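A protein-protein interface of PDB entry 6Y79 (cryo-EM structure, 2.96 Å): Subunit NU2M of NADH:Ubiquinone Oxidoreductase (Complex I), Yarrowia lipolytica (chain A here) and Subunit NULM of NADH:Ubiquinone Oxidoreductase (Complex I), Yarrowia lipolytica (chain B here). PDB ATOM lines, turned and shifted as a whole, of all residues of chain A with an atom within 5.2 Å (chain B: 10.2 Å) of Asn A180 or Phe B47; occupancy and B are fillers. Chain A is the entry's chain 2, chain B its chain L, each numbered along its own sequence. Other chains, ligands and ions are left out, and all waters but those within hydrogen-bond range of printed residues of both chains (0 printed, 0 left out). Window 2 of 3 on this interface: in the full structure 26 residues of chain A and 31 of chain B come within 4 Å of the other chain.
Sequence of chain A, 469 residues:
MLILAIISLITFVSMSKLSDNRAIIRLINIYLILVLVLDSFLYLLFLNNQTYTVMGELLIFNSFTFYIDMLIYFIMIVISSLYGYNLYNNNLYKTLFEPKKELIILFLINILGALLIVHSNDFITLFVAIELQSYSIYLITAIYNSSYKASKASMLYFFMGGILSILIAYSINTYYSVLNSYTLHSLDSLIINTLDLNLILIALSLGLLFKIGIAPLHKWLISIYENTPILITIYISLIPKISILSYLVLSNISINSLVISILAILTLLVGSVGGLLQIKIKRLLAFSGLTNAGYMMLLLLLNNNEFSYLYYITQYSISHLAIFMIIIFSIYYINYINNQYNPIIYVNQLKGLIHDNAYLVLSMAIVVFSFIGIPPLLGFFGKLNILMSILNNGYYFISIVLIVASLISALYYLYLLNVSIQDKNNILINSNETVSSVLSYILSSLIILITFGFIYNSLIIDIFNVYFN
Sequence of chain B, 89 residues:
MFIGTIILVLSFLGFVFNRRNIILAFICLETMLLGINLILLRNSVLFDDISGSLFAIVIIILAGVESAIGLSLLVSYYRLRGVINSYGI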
ATOM      1  N   TYR A 176      -7.757   8.249  31.232  1.00  0.00           N
ATOM      2  CA  TYR A 176      -8.691   7.701  30.259  1.00  0.00           C
ATOM      3  C   TYR A 176      -9.968   8.524  30.171  1.00  0.00           C
ATOM      4  O   TYR A 176     -10.589   8.587  29.107  1.00  0.00           O
ATOM      5  CB  TYR A 176      -9.007   6.258  30.628  1.00  0.00           C
ATOM      6  CG  TYR A 176     -10.013   5.603  29.728  1.00  0.00           C
ATOM      7  CD1 TYR A 176      -9.665   5.204  28.451  1.00  0.00           C
ATOM      8  CD2 TYR A 176     -11.311   5.383  30.158  1.00  0.00           C
ATOM      9  CE1 TYR A 176     -10.576   4.613  27.632  1.00  0.00           C
ATOM     10  CE2 TYR A 176     -12.229   4.798  29.345  1.00  0.00           C
ATOM     11  CZ  TYR A 176     -11.858   4.415  28.087  1.00  0.00           C
ATOM     12  OH  TYR A 176     -12.785   3.822  27.285  1.00  0.00           O
ATOM     13  N   SER A 177     -10.371   9.154  31.275  1.00  0.00           N
ATOM     14  CA  SER A 177     -11.605   9.924  31.306  1.00  0.00           C
ATOM     15  C   SER A 177     -11.508  11.230  30.524  1.00  0.00           C
ATOM     16  O   SER A 177     -12.544  11.813  30.194  1.00  0.00           O
ATOM     17  CB  SER A 177     -11.979  10.223  32.758  1.00  0.00           C
ATOM     18  OG  SER A 177     -12.072   9.051  33.521  1.00  0.00           O
ATOM     19  N   VAL A 178     -10.304  11.721  30.246  1.00  0.00           N
ATOM     20  CA  VAL A 178     -10.139  12.938  29.468  1.00  0.00           C
ATOM     21  C   VAL A 178      -9.614  12.664  28.072  1.00  0.00           C
ATOM     22  O   VAL A 178      -9.773  13.518  27.192  1.00  0.00           O
ATOM     23  CB  VAL A 178      -9.232  13.952  30.195  1.00  0.00           C
ATOM     24  CG1 VAL A 178      -9.749  14.214  31.589  1.00  0.00           C
ATOM     25  CG2 VAL A 178      -7.820  13.461  30.254  1.00  0.00           C
ATOM     26  N   LEU A 179      -9.004  11.514  27.837  1.00  0.00           N
ATOM     27  CA  LEU A 179      -8.529  11.114  26.526  1.00  0.00           C
ATOM     28  C   LEU A 179      -8.931   9.671  26.332  1.00  0.00           C
ATOM     29  O   LEU A 179      -8.553   8.813  27.132  1.00  0.00           O
ATOM     30  CB  LEU A 179      -7.012  11.238  26.413  1.00  0.00           C
ATOM     31  CG  LEU A 179      -6.367  12.612  26.407  1.00  0.00           C
ATOM     32  CD1 LEU A 179      -4.870  12.457  26.414  1.00  0.00           C
ATOM     33  CD2 LEU A 179      -6.820  13.375  25.186  1.00  0.00           C
ATOM     34  N   ASN A 180      -9.666   9.385  25.271  1.00  0.00           N
ATOM     35  CA  ASN A 180     -10.003   8.001  24.969  1.00  0.00           C
ATOM     36  C   ASN A 180      -8.749   7.340  24.393  1.00  0.00           C
ATOM     37  O   ASN A 180      -8.598   7.152  23.183  1.00  0.00           O
ATOM     38  CB  ASN A 180     -11.191   7.953  24.023  1.00  0.00           C
ATOM     39  CG  ASN A 180     -11.801   6.599  23.931  1.00  0.00           C
ATOM     40  OD1 ASN A 180     -11.234   5.623  24.405  1.00  0.00           O
ATOM     41  ND2 ASN A 180     -12.966   6.518  23.315  1.00  0.00           N
ATOM     42  N   SER A 181      -7.843   6.960  25.296  1.00  0.00           N
ATOM     43  CA  SER A 181      -6.520   6.487  24.916  1.00  0.00           C
ATOM     44  C   SER A 181      -5.876   5.804  26.106  1.00  0.00           C
ATOM     45  O   SER A 181      -6.279   5.999  27.252  1.00  0.00           O
ATOM     46  CB  SER A 181      -5.628   7.634  24.428  1.00  0.00           C
ATOM     47  OG  SER A 181      -4.471   7.138  23.788  1.00  0.00           O
ATOM     48  N   TYR A 182      -4.858   4.997  25.807  1.00  0.00           N
ATOM     49  CA  TYR A 182      -4.003   4.378  26.807  1.00  0.00           C
ATOM     50  C   TYR A 182      -2.543   4.690  26.632  1.00  0.00           C
ATOM     51  O   TYR A 182      -1.756   4.393  27.531  1.00  0.00           O
ATOM     52  CB  TYR A 182      -4.125   2.857  26.765  1.00  0.00           C
ATOM     53  CG  TYR A 182      -5.326   2.364  27.459  1.00  0.00           C
ATOM     54  CD1 TYR A 182      -5.790   3.003  28.595  1.00  0.00           C
ATOM     55  CD2 TYR A 182      -6.003   1.258  26.992  1.00  0.00           C
ATOM     56  CE1 TYR A 182      -6.895   2.557  29.242  1.00  0.00           C
ATOM     57  CE2 TYR A 182      -7.111   0.804  27.634  1.00  0.00           C
ATOM     58  CZ  TYR A 182      -7.555   1.458  28.752  1.00  0.00           C
ATOM     59  OH  TYR A 182      -8.668   1.004  29.399  1.00  0.00           O
ATOM     60  N   ILE B  39     -15.927   4.307  38.461  1.00  0.00           N
ATOM     61  CA  ILE B  39     -15.527   5.458  37.646  1.00  0.00           C
ATOM     62  C   ILE B  39     -15.172   5.025  36.228  1.00  0.00           C
ATOM     63  O   ILE B  39     -15.623   5.626  35.236  1.00  0.00           O
ATOM     64  CB  ILE B  39     -14.351   6.191  38.313  1.00  0.00           C
ATOM     65  CG1 ILE B  39     -14.751   6.713  39.682  1.00  0.00           C
ATOM     66  CG2 ILE B  39     -13.884   7.339  37.459  1.00  0.00           C
ATOM     67  CD1 ILE B  39     -13.606   7.225  40.489  1.00  0.00           C
ATOM     68  N   LEU B  40     -14.423   3.930  36.112  1.00  0.00           N
ATOM     69  CA  LEU B  40     -13.964   3.492  34.801  1.00  0.00           C
ATOM     70  C   LEU B  40     -15.101   2.963  33.932  1.00  0.00           C
ATOM     71  O   LEU B  40     -15.155   3.249  32.729  1.00  0.00           O
ATOM     72  CB  LEU B  40     -12.901   2.428  34.981  1.00  0.00           C
ATOM     73  CG  LEU B  40     -12.384   1.860  33.688  1.00  0.00           C
ATOM     74  CD1 LEU B  40     -11.671   2.938  32.905  1.00  0.00           C
ATOM     75  CD2 LEU B  40     -11.484   0.788  34.095  1.00  0.00           C
ATOM     76  N   LEU B  41     -16.018   2.191  34.520  1.00  0.00           N
ATOM     77  CA  LEU B  41     -17.097   1.615  33.728  1.00  0.00           C
ATOM     78  C   LEU B  41     -18.099   2.673  33.302  1.00  0.00           C
ATOM     79  O   LEU B  41     -18.667   2.589  32.201  1.00  0.00           O
ATOM     80  CB  LEU B  41     -17.771   0.492  34.503  1.00  0.00           C
ATOM     81  CG  LEU B  41     -16.963  -0.795  34.450  1.00  0.00           C
ATOM     82  CD1 LEU B  41     -17.647  -1.860  35.241  1.00  0.00           C
ATOM     83  CD2 LEU B  41     -16.796  -1.239  33.016  1.00  0.00           C
ATOM     84  N   ARG B  42     -18.291   3.707  34.131  1.00  0.00           N
ATOM     85  CA  ARG B  42     -19.074   4.849  33.677  1.00  0.00           C
ATOM     86  C   ARG B  42     -18.417   5.542  32.486  1.00  0.00           C
ATOM     87  O   ARG B  42     -19.100   5.893  31.521  1.00  0.00           O
ATOM     88  CB  ARG B  42     -19.284   5.840  34.815  1.00  0.00           C
ATOM     89  CG  ARG B  42     -20.199   6.980  34.433  1.00  0.00           C
ATOM     90  CD  ARG B  42     -19.828   8.227  35.162  1.00  0.00           C
ATOM     91  NE  ARG B  42     -20.595   9.381  34.718  1.00  0.00           N
ATOM     92  CZ  ARG B  42     -20.186  10.228  33.783  1.00  0.00           C
ATOM     93  NH1 ARG B  42     -19.011  10.047  33.201  1.00  0.00           N
ATOM     94  NH2 ARG B  42     -20.949  11.256  33.436  1.00  0.00           N
ATOM     95  N   ASN B  43     -17.091   5.714  32.515  1.00  0.00           N
ATOM     96  CA  ASN B  43     -16.410   6.364  31.389  1.00  0.00           C
ATOM     97  C   ASN B  43     -16.474   5.525  30.116  1.00  0.00           C
ATOM     98  O   ASN B  43     -16.551   6.069  29.007  1.00  0.00           O
ATOM     99  CB  ASN B  43     -14.957   6.639  31.765  1.00  0.00           C
ATOM    100  CG  ASN B  43     -14.830   7.767  32.739  1.00  0.00           C
ATOM    101  OD1 ASN B  43     -15.491   8.796  32.593  1.00  0.00           O
ATOM    102  ND2 ASN B  43     -14.008   7.588  33.760  1.00  0.00           N
ATOM    103  N   SER B  44     -16.439   4.203  30.262  1.00  0.00           N
ATOM    104  CA  SER B  44     -16.567   3.310  29.115  1.00  0.00           C
ATOM    105  C   SER B  44     -17.951   3.406  28.490  1.00  0.00           C
ATOM    106  O   SER B  44     -18.094   3.368  27.262  1.00  0.00           O
ATOM    107  CB  SER B  44     -16.283   1.876  29.548  1.00  0.00           C
ATOM    108  OG  SER B  44     -16.453   0.974  28.475  1.00  0.00           O
ATOM    109  N   VAL B  45     -18.986   3.507  29.328  1.00  0.00           N
ATOM    110  CA  VAL B  45     -20.348   3.663  28.821  1.00  0.00           C
ATOM    111  C   VAL B  45     -20.520   5.011  28.134  1.00  0.00           C
ATOM    112  O   VAL B  45     -21.115   5.102  27.053  1.00  0.00           O
ATOM    113  CB  VAL B  45     -21.350   3.469  29.972  1.00  0.00           C
ATOM    114  CG1 VAL B  45     -22.723   4.004  29.626  1.00  0.00           C
ATOM    115  CG2 VAL B  45     -21.445   2.018  30.304  1.00  0.00           C
ATOM    116  N   LEU B  46     -19.974   6.071  28.725  1.00  0.00           N
ATOM    117  CA  LEU B  46     -20.116   7.398  28.138  1.00  0.00           C
ATOM    118  C   LEU B  46     -19.312   7.574  26.854  1.00  0.00           C
ATOM    119  O   LEU B  46     -19.732   8.341  25.987  1.00  0.00           O
ATOM    120  CB  LEU B  46     -19.715   8.486  29.142  1.00  0.00           C
ATOM    121  CG  LEU B  46     -20.749   9.134  30.069  1.00  0.00           C
ATOM    122  CD1 LEU B  46     -21.839   9.802  29.265  1.00  0.00           C
ATOM    123  CD2 LEU B  46     -21.335   8.175  31.050  1.00  0.00           C
ATOM    124  N   PHE B  47     -18.183   6.883  26.694  1.00  0.00           N
ATOM    125  CA  PHE B  47     -17.362   7.054  25.499  1.00  0.00           C
ATOM    126  C   PHE B  47     -17.699   6.069  24.393  1.00  0.00           C
ATOM    127  O   PHE B  47     -17.096   6.161  23.318  1.00  0.00           O
ATOM    128  CB  PHE B  47     -15.872   6.918  25.831  1.00  0.00           C
ATOM    129  CG  PHE B  47     -15.329   8.025  26.682  1.00  0.00           C
ATOM    130  CD1 PHE B  47     -15.979   9.243  26.768  1.00  0.00           C
ATOM    131  CD2 PHE B  47     -14.173   7.838  27.410  1.00  0.00           C
ATOM    132  CE1 PHE B  47     -15.487  10.243  27.561  1.00  0.00           C
ATOM    133  CE2 PHE B  47     -13.679   8.837  28.201  1.00  0.00           C
ATOM    134  CZ  PHE B  47     -14.335  10.040  28.274  1.00  0.00           C
ATOM    135  N   ASP B  48     -18.616   5.124  24.656  1.00  0.00           N
ATOM    136  CA  ASP B  48     -19.070   4.079  23.724  1.00  0.00           C
ATOM    137  C   ASP B  48     -17.926   3.138  23.328  1.00  0.00           C
ATOM    138  O   ASP B  48     -17.749   2.817  22.160  1.00  0.00           O
ATOM    139  CB  ASP B  48     -19.751   4.695  22.484  1.00  0.00           C
ATOM    140  CG  ASP B  48     -20.560   3.691  21.659  1.00  0.00           C
ATOM    141  OD1 ASP B  48     -20.713   2.534  22.092  1.00  0.00           O
ATOM    142  OD2 ASP B  48     -21.006   4.058  20.553  1.00  0.00           O
ATOM    143  N   ASP B  49     -17.162   2.656  24.305  1.00  0.00           N
ATOM    144  CA  ASP B  49     -16.111   1.715  23.943  1.00  0.00           C
ATOM    145  C   ASP B  49     -15.842   0.700  25.043  1.00  0.00           C
ATOM    146  O   ASP B  49     -16.230   0.870  26.198  1.00  0.00           O
ATOM    147  CB  ASP B  49     -14.816   2.427  23.586  1.00  0.00           C
ATOM    148  CG  ASP B  49     -14.286   3.249  24.704  1.00  0.00           C
ATOM    149  OD1 ASP B  49     -15.016   3.541  25.667  1.00  0.00           O
ATOM    150  OD2 ASP B  49     -13.101   3.583  24.641  1.00  0.00           O
ATOM    151  N   ILE B  50     -15.147  -0.367  24.644  1.00  0.00           N
ATOM    152  CA  ILE B  50     -14.865  -1.517  25.495  1.00  0.00           C
ATOM    153  C   ILE B  50     -13.559  -1.433  26.250  1.00  0.00           C
ATOM    154  O   ILE B  50     -13.207  -2.394  26.947  1.00  0.00           O
ATOM    155  CB  ILE B  50     -14.644  -2.821  24.721  1.00  0.00           C
ATOM    156  CG1 ILE B  50     -13.682  -2.491  23.595  1.00  0.00           C
ATOM    157  CG2 ILE B  50     -15.930  -3.405  24.242  1.00  0.00           C
ATOM    158  CD1 ILE B  50     -12.875  -3.604  23.229  1.00  0.00           C
ATOM    159  N   SER B  51     -12.779  -0.375  26.065  1.00  0.00           N
ATOM    160  CA  SER B  51     -11.387  -0.456  26.475  1.00  0.00           C
ATOM    161  C   SER B  51     -11.267  -0.160  27.954  1.00  0.00           C
ATOM    162  O   SER B  51     -10.415  -0.731  28.653  1.00  0.00           O
ATOM    163  CB  SER B  51     -10.544   0.499  25.642  1.00  0.00           C
ATOM    164  OG  SER B  51      -9.277  -0.051  25.491  1.00  0.00           O
ATOM    165  N   GLY B  52     -12.124   0.736  28.439  1.00  0.00           N
ATOM    166  CA  GLY B  52     -12.369   0.822  29.860  1.00  0.00           C
ATOM    167  C   GLY B  52     -12.987  -0.439  30.426  1.00  0.00           C
ATOM    168  O   GLY B  52     -12.650  -0.844  31.538  1.00  0.00           O
ATOM    169  N   SER B  53     -13.845  -1.117  29.653  1.00  0.00           N
ATOM    170  CA  SER B  53     -14.370  -2.406  30.095  1.00  0.00           C
ATOM    171  C   SER B  53     -13.272  -3.464  30.116  1.00  0.00           C
ATOM    172  O   SER B  53     -13.297  -4.363  30.958  1.00  0.00           O
ATOM    173  CB  SER B  53     -15.520  -2.841  29.190  1.00  0.00           C
ATOM    174  OG  SER B  53     -16.654  -2.011  29.352  1.00  0.00           O
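Among the printed residues, pairs that only touch across the chains: Tyr A176 with Leu B40, Tyr A176 with Phe B47, Ser A177 with Phe B47, Asn A180 with Phe B47 and Tyr A182 with Gly B52.
The side-chain amide nitrogen (ND2) of Asn B43 is in hydrogen-bond range of the backbone carbonyl oxygen (O) of Ile B39 (2.9 Å). The backbone carbonyl oxygen of Ser B44 lies within hydrogen-bond range of the backbone NH of Asp B49, at 3.2 Å.
ND2 of Asn B43 is in hydrogen-bond range of OG of Ser A177 (2.4 Å). OH of Tyr A176 sits at hydrogen-bond distance from OD2 of Asp B49 (2.7 Å). OD2 of Asp B49 sits close to OD1 of Asn A180. O of Ser B51 lies within hydrogen-bond range of OH of Tyr A182, at 2.6 Å. The backbone NH (N) of Gly B52 sits at hydrogen-bond distance from the side-chain hydroxyl (OH) of Tyr A176 (3.4 Å).
No residue of chain B comes within 4 Å of Leu A179. Asn A180 touches two residues of chain B. No residue of chain B comes within 4 Å of Ser A181. Of the printed residues of chain B, Tyr A182 touches Ser B51 and Gly B52. Printed residues of chain A within 4 Å of Leu B40: Tyr A176 (3.7 Å). Ser B44 touches none of the printed residues of chain A. Val B45 touches none of the printed residues of chain A. Phe B47 touches just these residues of chain A: Tyr A176 (3.2 Å), Ser A177 (3.2 Å) and Asn A180 (3.9 Å). Of the printed residues of chain A, Asp B49 touches Tyr A176 (2.7 Å) and Asn A180 (2.8 Å). Printed residues of chain A within 4 Å of Ser B51: Tyr A182. Of the printed residues of chain A, Gly B52 touches Tyr A176 (3.4 Å) and Tyr A182 (3.6 Å).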
